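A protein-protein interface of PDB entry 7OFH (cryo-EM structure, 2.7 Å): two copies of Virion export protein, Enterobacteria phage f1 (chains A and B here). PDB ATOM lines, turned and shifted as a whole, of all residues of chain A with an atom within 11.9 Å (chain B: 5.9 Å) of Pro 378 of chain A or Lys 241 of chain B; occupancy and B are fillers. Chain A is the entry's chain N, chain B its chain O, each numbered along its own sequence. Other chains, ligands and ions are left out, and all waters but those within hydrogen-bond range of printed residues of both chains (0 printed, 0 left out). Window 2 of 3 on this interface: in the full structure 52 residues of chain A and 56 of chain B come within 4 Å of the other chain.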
ATOM      1  N   PHE A 196      10.538  16.855   5.298  1.00  0.00           N
ATOM      2  CA  PHE A 196       9.509  16.412   6.227  1.00  0.00           C
ATOM      3  C   PHE A 196      10.178  16.041   7.531  1.00  0.00           C
ATOM      4  O   PHE A 196       9.924  14.979   8.074  1.00  0.00           O
ATOM      5  CB  PHE A 196       8.793  15.161   5.721  1.00  0.00           C
ATOM      6  CG  PHE A 196       7.744  14.591   6.640  1.00  0.00           C
ATOM      7  CD1 PHE A 196       6.515  15.215   6.801  1.00  0.00           C
ATOM      8  CD2 PHE A 196       7.974  13.403   7.323  1.00  0.00           C
ATOM      9  CE1 PHE A 196       5.549  14.683   7.648  1.00  0.00           C
ATOM     10  CE2 PHE A 196       7.012  12.869   8.170  1.00  0.00           C
ATOM     11  CZ  PHE A 196       5.799  13.509   8.329  1.00  0.00           C
ATOM     12  N   SER A 372      15.988  12.874 -10.072  1.00  0.00           N
ATOM     13  CA  SER A 372      15.121  12.531  -8.947  1.00  0.00           C
ATOM     14  C   SER A 372      15.937  11.955  -7.795  1.00  0.00           C
ATOM     15  O   SER A 372      16.757  11.073  -8.013  1.00  0.00           O
ATOM     16  CB  SER A 372      14.099  11.520  -9.360  1.00  0.00           C
ATOM     17  OG  SER A 372      13.338  11.108  -8.235  1.00  0.00           O
ATOM     18  N   GLN A 373      15.680  12.413  -6.572  1.00  0.00           N
ATOM     19  CA  GLN A 373      16.500  12.070  -5.417  1.00  0.00           C
ATOM     20  C   GLN A 373      15.580  11.905  -4.210  1.00  0.00           C
ATOM     21  O   GLN A 373      14.472  12.441  -4.222  1.00  0.00           O
ATOM     22  CB  GLN A 373      17.468  13.223  -5.193  1.00  0.00           C
ATOM     23  CG  GLN A 373      18.551  12.953  -4.175  1.00  0.00           C
ATOM     24  CD  GLN A 373      19.654  13.978  -4.287  1.00  0.00           C
ATOM     25  OE1 GLN A 373      19.852  14.594  -5.334  1.00  0.00           O
ATOM     26  NE2 GLN A 373      20.395  14.167  -3.203  1.00  0.00           N
ATOM     27  N   ASP A 374      16.011  11.165  -3.177  1.00  0.00           N
ATOM     28  CA  ASP A 374      15.102  10.784  -2.103  1.00  0.00           C
ATOM     29  C   ASP A 374      15.860  10.150  -0.940  1.00  0.00           C
ATOM     30  O   ASP A 374      15.997   8.927  -0.902  1.00  0.00           O
ATOM     31  CB  ASP A 374      14.075   9.752  -2.586  1.00  0.00           C
ATOM     32  CG  ASP A 374      12.670   9.944  -2.032  1.00  0.00           C
ATOM     33  OD1 ASP A 374      12.545  10.446  -0.891  1.00  0.00           O
ATOM     34  OD2 ASP A 374      11.705   9.596  -2.751  1.00  0.00           O
ATOM     35  N   SER A 375      16.310  10.966   0.021  1.00  0.00           N
ATOM     36  CA  SER A 375      16.865  10.416   1.251  1.00  0.00           C
ATOM     37  C   SER A 375      15.744  10.209   2.262  1.00  0.00           C
ATOM     38  O   SER A 375      14.946  11.107   2.482  1.00  0.00           O
ATOM     39  CB  SER A 375      17.970  11.270   1.816  1.00  0.00           C
ATOM     40  OG  SER A 375      17.564  12.622   1.879  1.00  0.00           O
ATOM     41  N   GLY A 376      15.688   9.019   2.868  1.00  0.00           N
ATOM     42  CA  GLY A 376      14.648   8.713   3.838  1.00  0.00           C
ATOM     43  C   GLY A 376      15.163   7.930   5.043  1.00  0.00           C
ATOM     44  O   GLY A 376      16.353   7.966   5.363  1.00  0.00           O
ATOM     45  N   VAL A 377      14.223   7.256   5.717  1.00  0.00           N
ATOM     46  CA  VAL A 377      14.497   6.377   6.843  1.00  0.00           C
ATOM     47  C   VAL A 377      13.913   5.010   6.488  1.00  0.00           C
ATOM     48  O   VAL A 377      12.713   4.909   6.237  1.00  0.00           O
ATOM     49  CB  VAL A 377      13.923   6.924   8.171  1.00  0.00           C
ATOM     50  CG1 VAL A 377      14.182   5.979   9.339  1.00  0.00           C
ATOM     51  CG2 VAL A 377      14.415   8.330   8.505  1.00  0.00           C
ATOM     52  N   PRO A 378      14.736   3.933   6.442  1.00  0.00           N
ATOM     53  CA  PRO A 378      14.262   2.612   6.023  1.00  0.00           C
ATOM     54  C   PRO A 378      13.362   1.942   7.073  1.00  0.00           C
ATOM     55  O   PRO A 378      12.455   1.242   6.658  1.00  0.00           O
ATOM     56  CB  PRO A 378      15.559   1.809   5.846  1.00  0.00           C
ATOM     57  CG  PRO A 378      16.533   2.459   6.805  1.00  0.00           C
ATOM     58  CD  PRO A 378      16.166   3.929   6.795  1.00  0.00           C
ATOM     59  N   LEU A 388      14.394  11.606  15.891  1.00  0.00           N
ATOM     60  CA  LEU A 388      14.257  12.419  14.689  1.00  0.00           C
ATOM     61  C   LEU A 388      13.979  11.531  13.477  1.00  0.00           C
ATOM     62  O   LEU A 388      14.373  10.365  13.468  1.00  0.00           O
ATOM     63  CB  LEU A 388      15.552  13.210  14.472  1.00  0.00           C
ATOM     64  CG  LEU A 388      16.101  13.974  15.680  1.00  0.00           C
ATOM     65  CD1 LEU A 388      17.557  14.361  15.461  1.00  0.00           C
ATOM     66  CD2 LEU A 388      15.258  15.204  15.991  1.00  0.00           C
ATOM     67  N   LEU A 389      13.311  12.101  12.459  1.00  0.00           N
ATOM     68  CA  LEU A 389      13.060  11.407  11.209  1.00  0.00           C
ATOM     69  C   LEU A 389      13.099  12.396  10.060  1.00  0.00           C
ATOM     70  O   LEU A 389      12.061  12.617   9.444  1.00  0.00           O
ATOM     71  CB  LEU A 389      11.671  10.763  11.227  1.00  0.00           C
ATOM     72  CG  LEU A 389      11.383   9.709  12.294  1.00  0.00           C
ATOM     73  CD1 LEU A 389       9.898   9.366  12.325  1.00  0.00           C
ATOM     74  CD2 LEU A 389      12.218   8.453  12.078  1.00  0.00           C
ATOM     75  N   PHE A 390      14.269  12.965   9.750  1.00  0.00           N
ATOM     76  CA  PHE A 390      14.414  13.762   8.536  1.00  0.00           C
ATOM     77  C   PHE A 390      14.141  12.905   7.296  1.00  0.00           C
ATOM     78  O   PHE A 390      14.493  11.724   7.283  1.00  0.00           O
ATOM     79  CB  PHE A 390      15.802  14.399   8.486  1.00  0.00           C
ATOM     80  CG  PHE A 390      16.087  15.333   9.633  1.00  0.00           C
ATOM     81  CD1 PHE A 390      15.691  16.664   9.574  1.00  0.00           C
ATOM     82  CD2 PHE A 390      16.745  14.889  10.773  1.00  0.00           C
ATOM     83  CE1 PHE A 390      15.943  17.530  10.630  1.00  0.00           C
ATOM     84  CE2 PHE A 390      17.003  15.757  11.828  1.00  0.00           C
ATOM     85  CZ  PHE A 390      16.602  17.075  11.754  1.00  0.00           C
ATOM     86  N   SER A 391      13.496  13.491   6.268  1.00  0.00           N
ATOM     87  CA  SER A 391      13.031  12.736   5.106  1.00  0.00           C
ATOM     88  C   SER A 391      12.815  13.627   3.882  1.00  0.00           C
ATOM     89  O   SER A 391      11.678  13.852   3.468  1.00  0.00           O
ATOM     90  CB  SER A 391      11.778  11.936   5.421  1.00  0.00           C
ATOM     91  OG  SER A 391      11.170  11.429   4.237  1.00  0.00           O
ATOM     92  N   SER A 392      13.911  14.066   3.253  1.00  0.00           N
ATOM     93  CA  SER A 392      13.838  14.964   2.110  1.00  0.00           C
ATOM     94  C   SER A 392      13.493  14.212   0.825  1.00  0.00           C
ATOM     95  O   SER A 392      13.438  12.987   0.818  1.00  0.00           O
ATOM     96  CB  SER A 392      15.116  15.751   1.975  1.00  0.00           C
ATOM     97  OG  SER A 392      16.216  14.896   1.696  1.00  0.00           O
ATOM     98  N   ARG A 393      13.249  14.973  -0.258  1.00  0.00           N
ATOM     99  CA  ARG A 393      13.074  14.449  -1.605  1.00  0.00           C
ATOM    100  C   ARG A 393      13.193  15.575  -2.621  1.00  0.00           C
ATOM    101  O   ARG A 393      12.380  16.489  -2.603  1.00  0.00           O
ATOM    102  CB  ARG A 393      11.678  13.851  -1.755  1.00  0.00           C
ATOM    103  CG  ARG A 393      11.398  13.270  -3.123  1.00  0.00           C
ATOM    104  CD  ARG A 393      10.072  12.564  -2.989  1.00  0.00           C
ATOM    105  NE  ARG A 393       9.716  11.917  -4.243  1.00  0.00           N
ATOM    106  CZ  ARG A 393       9.154  12.520  -5.295  1.00  0.00           C
ATOM    107  NH1 ARG A 393       8.877  13.817  -5.264  1.00  0.00           N
ATOM    108  NH2 ARG A 393       8.878  11.822  -6.383  1.00  0.00           N
ATOM    109  N   SER A 394      14.176  15.492  -3.528  1.00  0.00           N
ATOM    110  CA  SER A 394      14.272  16.431  -4.641  1.00  0.00           C
ATOM    111  C   SER A 394      13.709  15.808  -5.914  1.00  0.00           C
ATOM    112  O   SER A 394      13.452  14.612  -5.952  1.00  0.00           O
ATOM    113  CB  SER A 394      15.676  16.921  -4.833  1.00  0.00           C
ATOM    114  OG  SER A 394      16.037  17.824  -3.796  1.00  0.00           O
ATOM    115  N   ALA B 191      21.703   3.401  -1.092  1.00  0.00           N
ATOM    116  CA  ALA B 191      22.657   3.425   0.006  1.00  0.00           C
ATOM    117  C   ALA B 191      21.921   3.093   1.306  1.00  0.00           C
ATOM    118  O   ALA B 191      20.701   3.222   1.353  1.00  0.00           O
ATOM    119  CB  ALA B 191      23.320   4.779   0.075  1.00  0.00           C
ATOM    120  N   LEU B 192      22.655   2.654   2.347  1.00  0.00           N
ATOM    121  CA  LEU B 192      22.042   2.335   3.629  1.00  0.00           C
ATOM    122  C   LEU B 192      23.059   2.381   4.761  1.00  0.00           C
ATOM    123  O   LEU B 192      23.369   1.342   5.336  1.00  0.00           O
ATOM    124  CB  LEU B 192      21.400   0.948   3.543  1.00  0.00           C
ATOM    125  CG  LEU B 192      20.319   0.636   4.580  1.00  0.00           C
ATOM    126  CD1 LEU B 192      19.139  -0.077   3.930  1.00  0.00           C
ATOM    127  CD2 LEU B 192      20.873  -0.188   5.743  1.00  0.00           C
ATOM    128  N   ASP B 193      23.532   3.572   5.141  1.00  0.00           N
ATOM    129  CA  ASP B 193      24.297   3.685   6.376  1.00  0.00           C
ATOM    130  C   ASP B 193      23.401   3.323   7.563  1.00  0.00           C
ATOM    131  O   ASP B 193      22.215   3.648   7.548  1.00  0.00           O
ATOM    132  CB  ASP B 193      24.913   5.076   6.510  1.00  0.00           C
ATOM    133  CG  ASP B 193      25.577   5.554   5.230  1.00  0.00           C
ATOM    134  OD1 ASP B 193      26.290   4.736   4.592  1.00  0.00           O
ATOM    135  OD2 ASP B 193      25.361   6.733   4.867  1.00  0.00           O
ATOM    136  N   ALA B 239      20.417   5.970  10.870  1.00  0.00           N
ATOM    137  CA  ALA B 239      20.202   5.288   9.598  1.00  0.00           C
ATOM    138  C   ALA B 239      20.218   6.309   8.461  1.00  0.00           C
ATOM    139  O   ALA B 239      20.472   7.493   8.691  1.00  0.00           O
ATOM    140  CB  ALA B 239      18.926   4.482   9.621  1.00  0.00           C
ATOM    141  N   LEU B 240      19.977   5.817   7.237  1.00  0.00           N
ATOM    142  CA  LEU B 240      19.897   6.587   6.003  1.00  0.00           C
ATOM    143  C   LEU B 240      19.486   5.627   4.897  1.00  0.00           C
ATOM    144  O   LEU B 240      19.898   4.466   4.896  1.00  0.00           O
ATOM    145  CB  LEU B 240      21.268   7.174   5.681  1.00  0.00           C
ATOM    146  CG  LEU B 240      21.393   8.685   5.818  1.00  0.00           C
ATOM    147  CD1 LEU B 240      22.852   9.080   6.005  1.00  0.00           C
ATOM    148  CD2 LEU B 240      20.810   9.386   4.599  1.00  0.00           C
ATOM    149  N   LYS B 241      18.670   6.109   3.965  1.00  0.00           N
ATOM    150  CA  LYS B 241      18.340   5.306   2.807  1.00  0.00           C
ATOM    151  C   LYS B 241      18.194   6.236   1.611  1.00  0.00           C
ATOM    152  O   LYS B 241      17.085   6.496   1.136  1.00  0.00           O
ATOM    153  CB  LYS B 241      17.106   4.452   3.077  1.00  0.00           C
ATOM    154  CG  LYS B 241      16.848   3.357   2.056  1.00  0.00           C
ATOM    155  CD  LYS B 241      15.448   2.784   2.157  1.00  0.00           C
ATOM    156  CE  LYS B 241      15.249   1.510   1.359  1.00  0.00           C
ATOM    157  NZ  LYS B 241      13.886   0.949   1.538  1.00  0.00           N
ATOM    158  N   THR B 242      19.337   6.736   1.135  1.00  0.00           N
ATOM    159  CA  THR B 242      19.362   7.612  -0.020  1.00  0.00           C
ATOM    160  C   THR B 242      19.141   6.801  -1.296  1.00  0.00           C
ATOM    161  O   THR B 242      19.958   5.946  -1.601  1.00  0.00           O
ATOM    162  CB  THR B 242      20.702   8.346  -0.085  1.00  0.00           C
ATOM    163  OG1 THR B 242      20.969   8.949   1.183  1.00  0.00           O
ATOM    164  CG2 THR B 242      20.731   9.402  -1.169  1.00  0.00           C
ATOM    165  N   ASN B 243      18.056   7.076  -2.032  1.00  0.00           N
ATOM    166  CA  ASN B 243      17.938   6.710  -3.437  1.00  0.00           C
ATOM    167  C   ASN B 243      18.311   7.884  -4.345  1.00  0.00           C
ATOM    168  O   ASN B 243      18.627   8.971  -3.865  1.00  0.00           O
ATOM    169  CB  ASN B 243      16.535   6.253  -3.785  1.00  0.00           C
ATOM    170  CG  ASN B 243      16.223   4.888  -3.222  1.00  0.00           C
ATOM    171  OD1 ASN B 243      17.126   4.111  -2.926  1.00  0.00           O
ATOM    172  ND2 ASN B 243      14.942   4.581  -3.086  1.00  0.00           N
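The backbone NH of Asn 243 of chain B sits at hydrogen-bond distance from the backbone carbonyl oxygen of Asp 374 of chain A, 3.0 Å away. The backbone NH (N) of Lys 241 of chain B lies within hydrogen-bond range of the backbone carbonyl oxygen (O) of Gly 376 of chain A (3.3 Å). The backbone carbonyl oxygen of Asp 374 of chain A sits close to the backbone carbonyl oxygen of Lys 241 of chain B, 3.4 Å away.
The backbone carbonyl oxygen of Gln 373 of chain A is in hydrogen-bond range of the backbone NH of Ser 394 of chain A (3.1 Å). OD2 of Asp 374 of chain A lies within salt-bridge range of NE of Arg 393 of chain A (3.4 Å). The side-chain hydroxyl of Ser 375 of chain A sits at hydrogen-bond distance from the side-chain hydroxyl of Ser 392 of chain A. O of Thr 242 of chain B is in hydrogen-bond range of N of Ala 191 of chain B, 3.1 Å away. The backbone carbonyl oxygen of Asp 193 of chain B lies within hydrogen-bond range of the backbone NH of Leu 240 of chain B (3.1 Å).
Gln 373 of chain A touches Asn 243 of chain B (CG to O, 3.99 Å). Thr 242 of chain B touches Asp 374 of chain A (CA to O, 3.7 Å). CA of Ser 375 of chain A touches O of Lys 241 of chain B (3.9 Å). Ser 375 of chain A touches Thr 242 of chain B (CB to OG1, 3.8 Å). Leu 240 of chain B touches Gly 376 of chain A (CA to O, 3.9 Å). Ala 239 of chain B touches Pro 378 of chain A. Pro 378 of chain A touches Lys 241 of chain B (CB to CD, 3.8 Å).
Printed residues of chain B within 4 Å of Gln 373 of chain A: Asn 243. Printed residues of chain B within 4 Å of Asp 374 of chain A: Lys 241 (3.4 Å), Thr 242 (3.7 Å) and Asn 243 (3.0 Å). Of the printed residues of chain B, Ser 375 of chain A touches Lys 241 (3.9 Å) and Thr 242 (3.8 Å). Of the printed residues of chain B, Gly 376 of chain A touches Leu 240 (3.9 Å) and Lys 241 (3.3 Å). Of the printed residues of chain B, Pro 378 of chain A touches Ala 239 (3.99 Å) and Lys 241 (3.8 Å). No residue of chain A comes within 4 Å of Leu 192 of chain B. No residue of chain A comes within 4 Å of Asp 193 of chain B. Of the printed residues of chain A, Ala 239 of chain B touches Pro 378. Leu 240 of chain B touches just one residue of chain A: Gly 376. Lys 241 of chain B touches just these residues of chain A: Asp 374, Ser 375, Gly 376 and Pro 378. The nearest printed residue of chain B that does not touch Pro 378 of chain A is Leu 240 of chain B (4.2 Å). The nearest printed residue of chain B that does not touch Gly 376 of chain A is Thr 242 of chain B (4.6 Å).
Printed residues of chain A that touch a printed residue of chain B: Gln 373, Asp 374, Ser 375, Gly 376 and Pro 378. Hydrophobic or aromatic side chains of chain A that line the printed part of chain B: Pro 378. Of the 8 printed residues of chain B, 5 touch a printed residue of chain A. Hydrophobic or aromatic side chains of chain B that line the printed part of chain A: Ala 239.
No position is printed for both chains. Of the 10 pairs that touch across the chains among the printed residues, none has its exchanged pair printed and touching as well.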
